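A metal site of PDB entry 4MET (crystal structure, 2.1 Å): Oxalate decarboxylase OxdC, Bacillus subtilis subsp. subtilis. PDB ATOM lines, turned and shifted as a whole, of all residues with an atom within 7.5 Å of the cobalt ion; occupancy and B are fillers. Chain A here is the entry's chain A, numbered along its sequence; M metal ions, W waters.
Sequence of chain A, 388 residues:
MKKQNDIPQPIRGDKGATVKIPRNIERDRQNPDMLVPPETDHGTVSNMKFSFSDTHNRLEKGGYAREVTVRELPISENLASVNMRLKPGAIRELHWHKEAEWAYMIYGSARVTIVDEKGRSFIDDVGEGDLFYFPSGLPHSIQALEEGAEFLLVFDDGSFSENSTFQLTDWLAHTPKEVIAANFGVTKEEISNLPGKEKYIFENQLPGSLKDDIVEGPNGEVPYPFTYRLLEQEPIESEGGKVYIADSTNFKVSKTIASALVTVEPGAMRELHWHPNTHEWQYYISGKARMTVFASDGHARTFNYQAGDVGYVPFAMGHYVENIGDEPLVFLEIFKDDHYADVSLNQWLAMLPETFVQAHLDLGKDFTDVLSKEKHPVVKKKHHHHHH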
ATOM      1  N   ARG A 270      27.675 -21.374 -11.914  1.00  0.00           N
ATOM      2  CA  ARG A 270      28.011 -19.954 -12.000  1.00  0.00           C
ATOM      3  C   ARG A 270      27.276 -19.324 -10.825  1.00  0.00           C
ATOM      4  O   ARG A 270      26.054 -19.478 -10.710  1.00  0.00           O
ATOM      5  CB  ARG A 270      27.512 -19.375 -13.336  1.00  0.00           C
ATOM      6  CG  ARG A 270      27.800 -17.898 -13.576  1.00  0.00           C
ATOM      7  CD  ARG A 270      29.288 -17.626 -13.764  1.00  0.00           C
ATOM      8  NE  ARG A 270      29.548 -16.209 -14.006  1.00  0.00           N
ATOM      9  CZ  ARG A 270      29.572 -15.268 -13.055  1.00  0.00           C
ATOM     10  NH1 ARG A 270      29.333 -15.590 -11.798  1.00  0.00           N
ATOM     11  NH2 ARG A 270      29.824 -13.994 -13.368  1.00  0.00           N
ATOM     12  N   GLU A 271      28.004 -18.640  -9.957  1.00  0.00           N
ATOM     13  CA  GLU A 271      27.461 -18.225  -8.657  1.00  0.00           C
ATOM     14  C   GLU A 271      26.371 -17.165  -8.803  1.00  0.00           C
ATOM     15  O   GLU A 271      26.196 -16.572  -9.869  1.00  0.00           O
ATOM     16  CB  GLU A 271      28.576 -17.673  -7.755  1.00  0.00           C
ATOM     17  CG  GLU A 271      29.250 -16.420  -8.322  1.00  0.00           C
ATOM     18  CD  GLU A 271      29.985 -15.631  -7.268  1.00  0.00           C
ATOM     19  OE1 GLU A 271      29.776 -15.906  -6.067  1.00  0.00           O
ATOM     20  OE2 GLU A 271      30.760 -14.720  -7.624  1.00  0.00           O
ATOM     21  N   HIS A 273      24.708 -13.799  -8.924  1.00  0.00           N
ATOM     22  CA  HIS A 273      25.217 -12.487  -9.274  1.00  0.00           C
ATOM     23  C   HIS A 273      24.189 -11.733 -10.113  1.00  0.00           C
ATOM     24  O   HIS A 273      23.139 -12.282 -10.487  1.00  0.00           O
ATOM     25  CB  HIS A 273      26.510 -12.636 -10.081  1.00  0.00           C
ATOM     26  CG  HIS A 273      26.309 -13.200 -11.451  1.00  0.00           C
ATOM     27  ND1 HIS A 273      26.039 -14.538 -11.671  1.00  0.00           N
ATOM     28  CD2 HIS A 273      26.309 -12.618 -12.674  1.00  0.00           C
ATOM     29  CE1 HIS A 273      25.884 -14.755 -12.970  1.00  0.00           C
ATOM     30  NE2 HIS A 273      26.053 -13.609 -13.601  1.00  0.00           N
ATOM     31  N   TRP A 274      24.489 -10.468 -10.393  1.00  0.00           N
ATOM     32  CA  TRP A 274      23.742  -9.722 -11.409  1.00  0.00           C
ATOM     33  C   TRP A 274      24.685  -8.809 -12.140  1.00  0.00           C
ATOM     34  O   TRP A 274      25.845  -8.641 -11.737  1.00  0.00           O
ATOM     35  CB  TRP A 274      22.574  -8.926 -10.824  1.00  0.00           C
ATOM     36  CG  TRP A 274      22.950  -7.721 -10.024  1.00  0.00           C
ATOM     37  CD1 TRP A 274      23.001  -6.431 -10.458  1.00  0.00           C
ATOM     38  CD2 TRP A 274      23.285  -7.693  -8.623  1.00  0.00           C
ATOM     39  NE1 TRP A 274      23.357  -5.598  -9.426  1.00  0.00           N
ATOM     40  CE2 TRP A 274      23.545  -6.352  -8.287  1.00  0.00           C
ATOM     41  CE3 TRP A 274      23.403  -8.679  -7.633  1.00  0.00           C
ATOM     42  CZ2 TRP A 274      23.910  -5.957  -6.991  1.00  0.00           C
ATOM     43  CZ3 TRP A 274      23.762  -8.292  -6.351  1.00  0.00           C
ATOM     44  CH2 TRP A 274      24.013  -6.934  -6.042  1.00  0.00           C
ATOM     45  N   HIS A 275      24.186  -8.232 -13.233  1.00  0.00           N
ATOM     46  CA  HIS A 275      24.949  -7.265 -14.016  1.00  0.00           C
ATOM     47  C   HIS A 275      24.355  -5.878 -13.842  1.00  0.00           C
ATOM     48  O   HIS A 275      23.174  -5.670 -14.119  1.00  0.00           O
ATOM     49  CB  HIS A 275      24.983  -7.736 -15.480  1.00  0.00           C
ATOM     50  CG  HIS A 275      25.497  -9.125 -15.610  1.00  0.00           C
ATOM     51  ND1 HIS A 275      26.836  -9.438 -15.449  1.00  0.00           N
ATOM     52  CD2 HIS A 275      24.860 -10.315 -15.761  1.00  0.00           C
ATOM     53  CE1 HIS A 275      27.003 -10.737 -15.550  1.00  0.00           C
ATOM     54  NE2 HIS A 275      25.819 -11.295 -15.739  1.00  0.00           N
ATOM     55  N   GLU A 280      21.834  -9.636 -20.216  1.00  0.00           N
ATOM     56  CA  GLU A 280      22.645 -10.774 -20.645  1.00  0.00           C
ATOM     57  C   GLU A 280      21.912 -11.650 -21.664  1.00  0.00           C
ATOM     58  O   GLU A 280      20.754 -12.022 -21.457  1.00  0.00           O
ATOM     59  CB  GLU A 280      23.003 -11.642 -19.443  1.00  0.00           C
ATOM     60  CG  GLU A 280      23.868 -12.842 -19.802  1.00  0.00           C
ATOM     61  CD  GLU A 280      24.354 -13.564 -18.570  1.00  0.00           C
ATOM     62  OE1 GLU A 280      24.903 -12.883 -17.678  1.00  0.00           O
ATOM     63  OE2 GLU A 280      24.186 -14.793 -18.498  1.00  0.00           O
ATOM     64  N   GLN A 282      22.395 -15.372 -23.700  1.00  0.00           N
ATOM     65  CA  GLN A 282      23.172 -16.592 -23.523  1.00  0.00           C
ATOM     66  C   GLN A 282      23.014 -17.573 -24.671  1.00  0.00           C
ATOM     67  O   GLN A 282      21.926 -17.700 -25.245  1.00  0.00           O
ATOM     68  CB  GLN A 282      22.736 -17.351 -22.255  1.00  0.00           C
ATOM     69  CG  GLN A 282      22.607 -16.514 -21.004  1.00  0.00           C
ATOM     70  CD  GLN A 282      21.992 -17.305 -19.859  1.00  0.00           C
ATOM     71  OE1 GLN A 282      21.165 -18.188 -20.082  1.00  0.00           O
ATOM     72  NE2 GLN A 282      22.384 -16.981 -18.627  1.00  0.00           N
ATOM     73  N   MET A 291      18.518 -22.190 -14.556  1.00  0.00           N
ATOM     74  CA  MET A 291      18.807 -20.853 -14.080  1.00  0.00           C
ATOM     75  C   MET A 291      17.505 -20.269 -13.592  1.00  0.00           C
ATOM     76  O   MET A 291      16.479 -20.395 -14.286  1.00  0.00           O
ATOM     77  CB  MET A 291      19.307 -19.963 -15.223  1.00  0.00           C
ATOM     78  CG  MET A 291      19.148 -18.451 -14.900  1.00  0.00           C
ATOM     79  SD  MET A 291      19.879 -17.400 -16.147  1.00  0.00           S
ATOM     80  CE  MET A 291      18.705 -17.682 -17.472  1.00  0.00           C
ATOM     81  N   VAL A 313      18.766 -12.746 -19.658  1.00  0.00           N
ATOM     82  CA  VAL A 313      18.569 -12.196 -18.310  1.00  0.00           C
ATOM     83  C   VAL A 313      18.462 -10.688 -18.408  1.00  0.00           C
ATOM     84  O   VAL A 313      19.483 -10.016 -18.620  1.00  0.00           O
ATOM     85  CB  VAL A 313      19.731 -12.517 -17.352  1.00  0.00           C
ATOM     86  CG1 VAL A 313      19.415 -11.983 -15.958  1.00  0.00           C
ATOM     87  CG2 VAL A 313      19.972 -14.004 -17.276  1.00  0.00           C
ATOM     88  N   MET A 317      18.753  -8.187 -13.212  1.00  0.00           N
ATOM     89  CA  MET A 317      18.038  -9.272 -12.560  1.00  0.00           C
ATOM     90  C   MET A 317      19.013 -10.303 -12.023  1.00  0.00           C
ATOM     91  O   MET A 317      20.031 -10.614 -12.658  1.00  0.00           O
ATOM     92  CB  MET A 317      17.027  -9.935 -13.501  1.00  0.00           C
ATOM     93  CG  MET A 317      15.966  -8.981 -14.041  1.00  0.00           C
ATOM     94  SD  MET A 317      14.528  -9.843 -14.720  1.00  0.00           S
ATOM     95  CE  MET A 317      13.455  -8.421 -15.005  1.00  0.00           C
ATOM     96  N   HIS A 319      20.637 -13.787 -10.980  1.00  0.00           N
ATOM     97  CA  HIS A 319      20.648 -15.108 -11.592  1.00  0.00           C
ATOM     98  C   HIS A 319      21.862 -15.944 -11.188  1.00  0.00           C
ATOM     99  O   HIS A 319      22.830 -15.437 -10.580  1.00  0.00           O
ATOM    100  CB  HIS A 319      20.554 -14.996 -13.123  1.00  0.00           C
ATOM    101  CG  HIS A 319      21.644 -14.176 -13.745  1.00  0.00           C
ATOM    102  ND1 HIS A 319      21.797 -12.830 -13.513  1.00  0.00           N
ATOM    103  CD2 HIS A 319      22.627 -14.519 -14.617  1.00  0.00           C
ATOM    104  CE1 HIS A 319      22.821 -12.362 -14.208  1.00  0.00           C
ATOM    105  NE2 HIS A 319      23.345 -13.370 -14.885  1.00  0.00           N
ATOM    106  N   TYR A 320      21.809 -17.225 -11.537  1.00  0.00           N
ATOM    107  CA  TYR A 320      22.908 -18.162 -11.359  1.00  0.00           C
ATOM    108  C   TYR A 320      22.732 -19.159 -12.504  1.00  0.00           C
ATOM    109  O   TYR A 320      21.651 -19.260 -13.089  1.00  0.00           O
ATOM    110  CB  TYR A 320      22.774 -18.881 -10.026  1.00  0.00           C
ATOM    111  CG  TYR A 320      21.550 -19.772  -9.983  1.00  0.00           C
ATOM    112  CD1 TYR A 320      21.594 -21.098 -10.412  1.00  0.00           C
ATOM    113  CD2 TYR A 320      20.335 -19.273  -9.526  1.00  0.00           C
ATOM    114  CE1 TYR A 320      20.459 -21.902 -10.395  1.00  0.00           C
ATOM    115  CE2 TYR A 320      19.205 -20.073  -9.485  1.00  0.00           C
ATOM    116  CZ  TYR A 320      19.267 -21.380  -9.927  1.00  0.00           C
ATOM    117  OH  TYR A 320      18.135 -22.154  -9.899  1.00  0.00           O
ATOM    118  N   VAL A 321      23.773 -19.909 -12.830  1.00  0.00           N
ATOM    119  CA  VAL A 321      23.597 -20.959 -13.844  1.00  0.00           C
ATOM    120  C   VAL A 321      24.181 -22.252 -13.297  1.00  0.00           C
ATOM    121  O   VAL A 321      25.392 -22.354 -13.087  1.00  0.00           O
ATOM    122  CB  VAL A 321      24.272 -20.580 -15.177  1.00  0.00           C
ATOM    123  CG1 VAL A 321      23.925 -21.619 -16.236  1.00  0.00           C
ATOM    124  CG2 VAL A 321      23.835 -19.179 -15.631  1.00  0.00           C
ATOM    125  N   PHE A 331      28.807 -22.450 -21.888  1.00  0.00           N
ATOM    126  CA  PHE A 331      27.897 -21.458 -22.453  1.00  0.00           C
ATOM    127  C   PHE A 331      28.553 -20.094 -22.633  1.00  0.00           C
ATOM    128  O   PHE A 331      29.546 -19.794 -21.967  1.00  0.00           O
ATOM    129  CB  PHE A 331      26.593 -21.359 -21.632  1.00  0.00           C
ATOM    130  CG  PHE A 331      26.782 -20.803 -20.245  1.00  0.00           C
ATOM    131  CD1 PHE A 331      26.547 -19.467 -19.979  1.00  0.00           C
ATOM    132  CD2 PHE A 331      27.139 -21.645 -19.193  1.00  0.00           C
ATOM    133  CE1 PHE A 331      26.695 -18.958 -18.718  1.00  0.00           C
ATOM    134  CE2 PHE A 331      27.296 -21.141 -17.912  1.00  0.00           C
ATOM    135  CZ  PHE A 331      27.072 -19.796 -17.663  1.00  0.00           C
ATOM    136  N   GLU A 333      28.099 -15.879 -22.537  1.00  0.00           N
ATOM    137  CA  GLU A 333      27.328 -14.741 -22.041  1.00  0.00           C
ATOM    138  C   GLU A 333      27.686 -13.566 -22.908  1.00  0.00           C
ATOM    139  O   GLU A 333      28.863 -13.274 -23.119  1.00  0.00           O
ATOM    140  CB  GLU A 333      27.687 -14.438 -20.596  1.00  0.00           C
ATOM    141  CG  GLU A 333      27.467 -15.604 -19.637  1.00  0.00           C
ATOM    142  CD  GLU A 333      28.234 -15.421 -18.354  1.00  0.00           C
ATOM    143  OE1 GLU A 333      29.295 -14.779 -18.402  1.00  0.00           O
ATOM    144  OE2 GLU A 333      27.783 -15.903 -17.289  1.00  0.00           O
ATOM    145  N   PHE A 335      26.937  -9.379 -23.838  1.00  0.00           N
ATOM    146  CA  PHE A 335      26.381  -8.107 -23.371  1.00  0.00           C
ATOM    147  C   PHE A 335      26.578  -7.025 -24.392  1.00  0.00           C
ATOM    148  O   PHE A 335      27.671  -6.885 -24.950  1.00  0.00           O
ATOM    149  CB  PHE A 335      27.029  -7.697 -22.052  1.00  0.00           C
ATOM    150  CG  PHE A 335      27.063  -8.790 -21.034  1.00  0.00           C
ATOM    151  CD1 PHE A 335      26.097  -8.861 -20.037  1.00  0.00           C
ATOM    152  CD2 PHE A 335      28.069  -9.749 -21.074  1.00  0.00           C
ATOM    153  CE1 PHE A 335      26.117  -9.878 -19.099  1.00  0.00           C
ATOM    154  CE2 PHE A 335      28.091 -10.778 -20.130  1.00  0.00           C
ATOM    155  CZ  PHE A 335      27.115 -10.836 -19.150  1.00  0.00           C
ATOM    156  N   TYR A 340      32.583  -6.000 -19.691  1.00  0.00           N
ATOM    157  CA  TYR A 340      31.922  -6.952 -18.797  1.00  0.00           C
ATOM    158  C   TYR A 340      31.956  -6.429 -17.372  1.00  0.00           C
ATOM    159  O   TYR A 340      32.959  -5.863 -16.922  1.00  0.00           O
ATOM    160  CB  TYR A 340      32.596  -8.338 -18.835  1.00  0.00           C
ATOM    161  CG  TYR A 340      31.975  -9.332 -17.878  1.00  0.00           C
ATOM    162  CD1 TYR A 340      30.921 -10.137 -18.267  1.00  0.00           C
ATOM    163  CD2 TYR A 340      32.431  -9.458 -16.571  1.00  0.00           C
ATOM    164  CE1 TYR A 340      30.325 -11.028 -17.409  1.00  0.00           C
ATOM    165  CE2 TYR A 340      31.843 -10.352 -15.692  1.00  0.00           C
ATOM    166  CZ  TYR A 340      30.783 -11.131 -16.137  1.00  0.00           C
ATOM    167  OH  TYR A 340      30.169 -12.022 -15.291  1.00  0.00           O
ATOM    168  N   ALA A 341      30.855  -6.613 -16.650  1.00  0.00           N
ATOM    169  CA  ALA A 341      30.822  -6.301 -15.230  1.00  0.00           C
ATOM    170  C   ALA A 341      29.751  -7.116 -14.541  1.00  0.00           C
ATOM    171  O   ALA A 341      28.631  -7.279 -15.066  1.00  0.00           O
ATOM    172  CB  ALA A 341      30.575  -4.823 -15.012  1.00  0.00           C
ATOM    173  N   ASP A 342      30.077  -7.626 -13.368  1.00  0.00           N
ATOM    174  CA  ASP A 342      29.071  -8.219 -12.501  1.00  0.00           C
ATOM    175  C   ASP A 342      29.212  -7.789 -11.034  1.00  0.00           C
ATOM    176  O   ASP A 342      30.250  -7.252 -10.632  1.00  0.00           O
ATOM    177  CB  ASP A 342      29.009  -9.763 -12.644  1.00  0.00           C
ATOM    178  CG  ASP A 342      30.273 -10.476 -12.139  1.00  0.00           C
ATOM    179  OD1 ASP A 342      30.859 -10.059 -11.133  1.00  0.00           O
ATOM    180  OD2 ASP A 342      30.646 -11.518 -12.737  1.00  0.00           O
HETATM  181 CO    CO M   1      25.522 -13.228 -15.709  1.00  0.00          CO
HETATM  182  O   HOH W   1      25.473 -15.486 -16.223  1.00  0.00           O
HETATM  183  O   HOH W   2      27.826 -13.428 -16.234  1.00  0.00           O
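The backbone carbonyl oxygen (O) of Glu 271 lies within hydrogen-bond range of a ring nitrogen (ND1) of His 273 (2.7 Å).
N of Val 313 lies within hydrogen-bond range of O of Glu 280.
The side-chain carboxylate (OE2) of Glu 280 is in hydrogen-bond range of the side-chain amide nitrogen (NE2) of Gln 282 (2.8 Å).
The side-chain carboxylate (OE2) of Glu 333 lies within salt-bridge range of the guanidinium group (NE) of Arg 270, 3.7 Å away.
A ring nitrogen (ND1) of His 275 is in hydrogen-bond range of the backbone carbonyl oxygen of Ala 341.
O of Met 317 sits at hydrogen-bond distance from ND1 of His 319, at 3.0 Å.
A ring nitrogen (ND1) of His 273 is in hydrogen-bond range of the guanidinium group (NH1) of Arg 270 (3.5 Å).
Glu 333 touches the cobalt ion (OE2 to CO, 3.8 Å).
Within 4 Å of the cobalt ion: His 273, His 275, Glu 280, His 319 and Glu 333.
Along chain A the residues within 4 Å of the cobalt ion span positions 273 to 333.
The cobalt ion is bound by a ring nitrogen (NE2) of His 275 (2.0 Å), the side-chain carboxylate (OE1) of Glu 280 (2.1 Å), a ring nitrogen (NE2) of His 273 (2.2 Å), water W1 (2.3 Å), a ring nitrogen (NE2) of His 319 (2.3 Å) and water W2 (2.4 Å).
The cobalt ion has six donor atoms within binding distance.
Water W2 bridges the side-chain carboxylate (OE2) of Glu 333 (2.7 Å) and the side-chain hydroxyl (OH) of Tyr 340 (2.9 Å).
Water W1 bridges the side-chain carboxylate of Glu 333 (2.6 Å) and the side-chain carboxylate of Glu 280 (2.7 Å).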
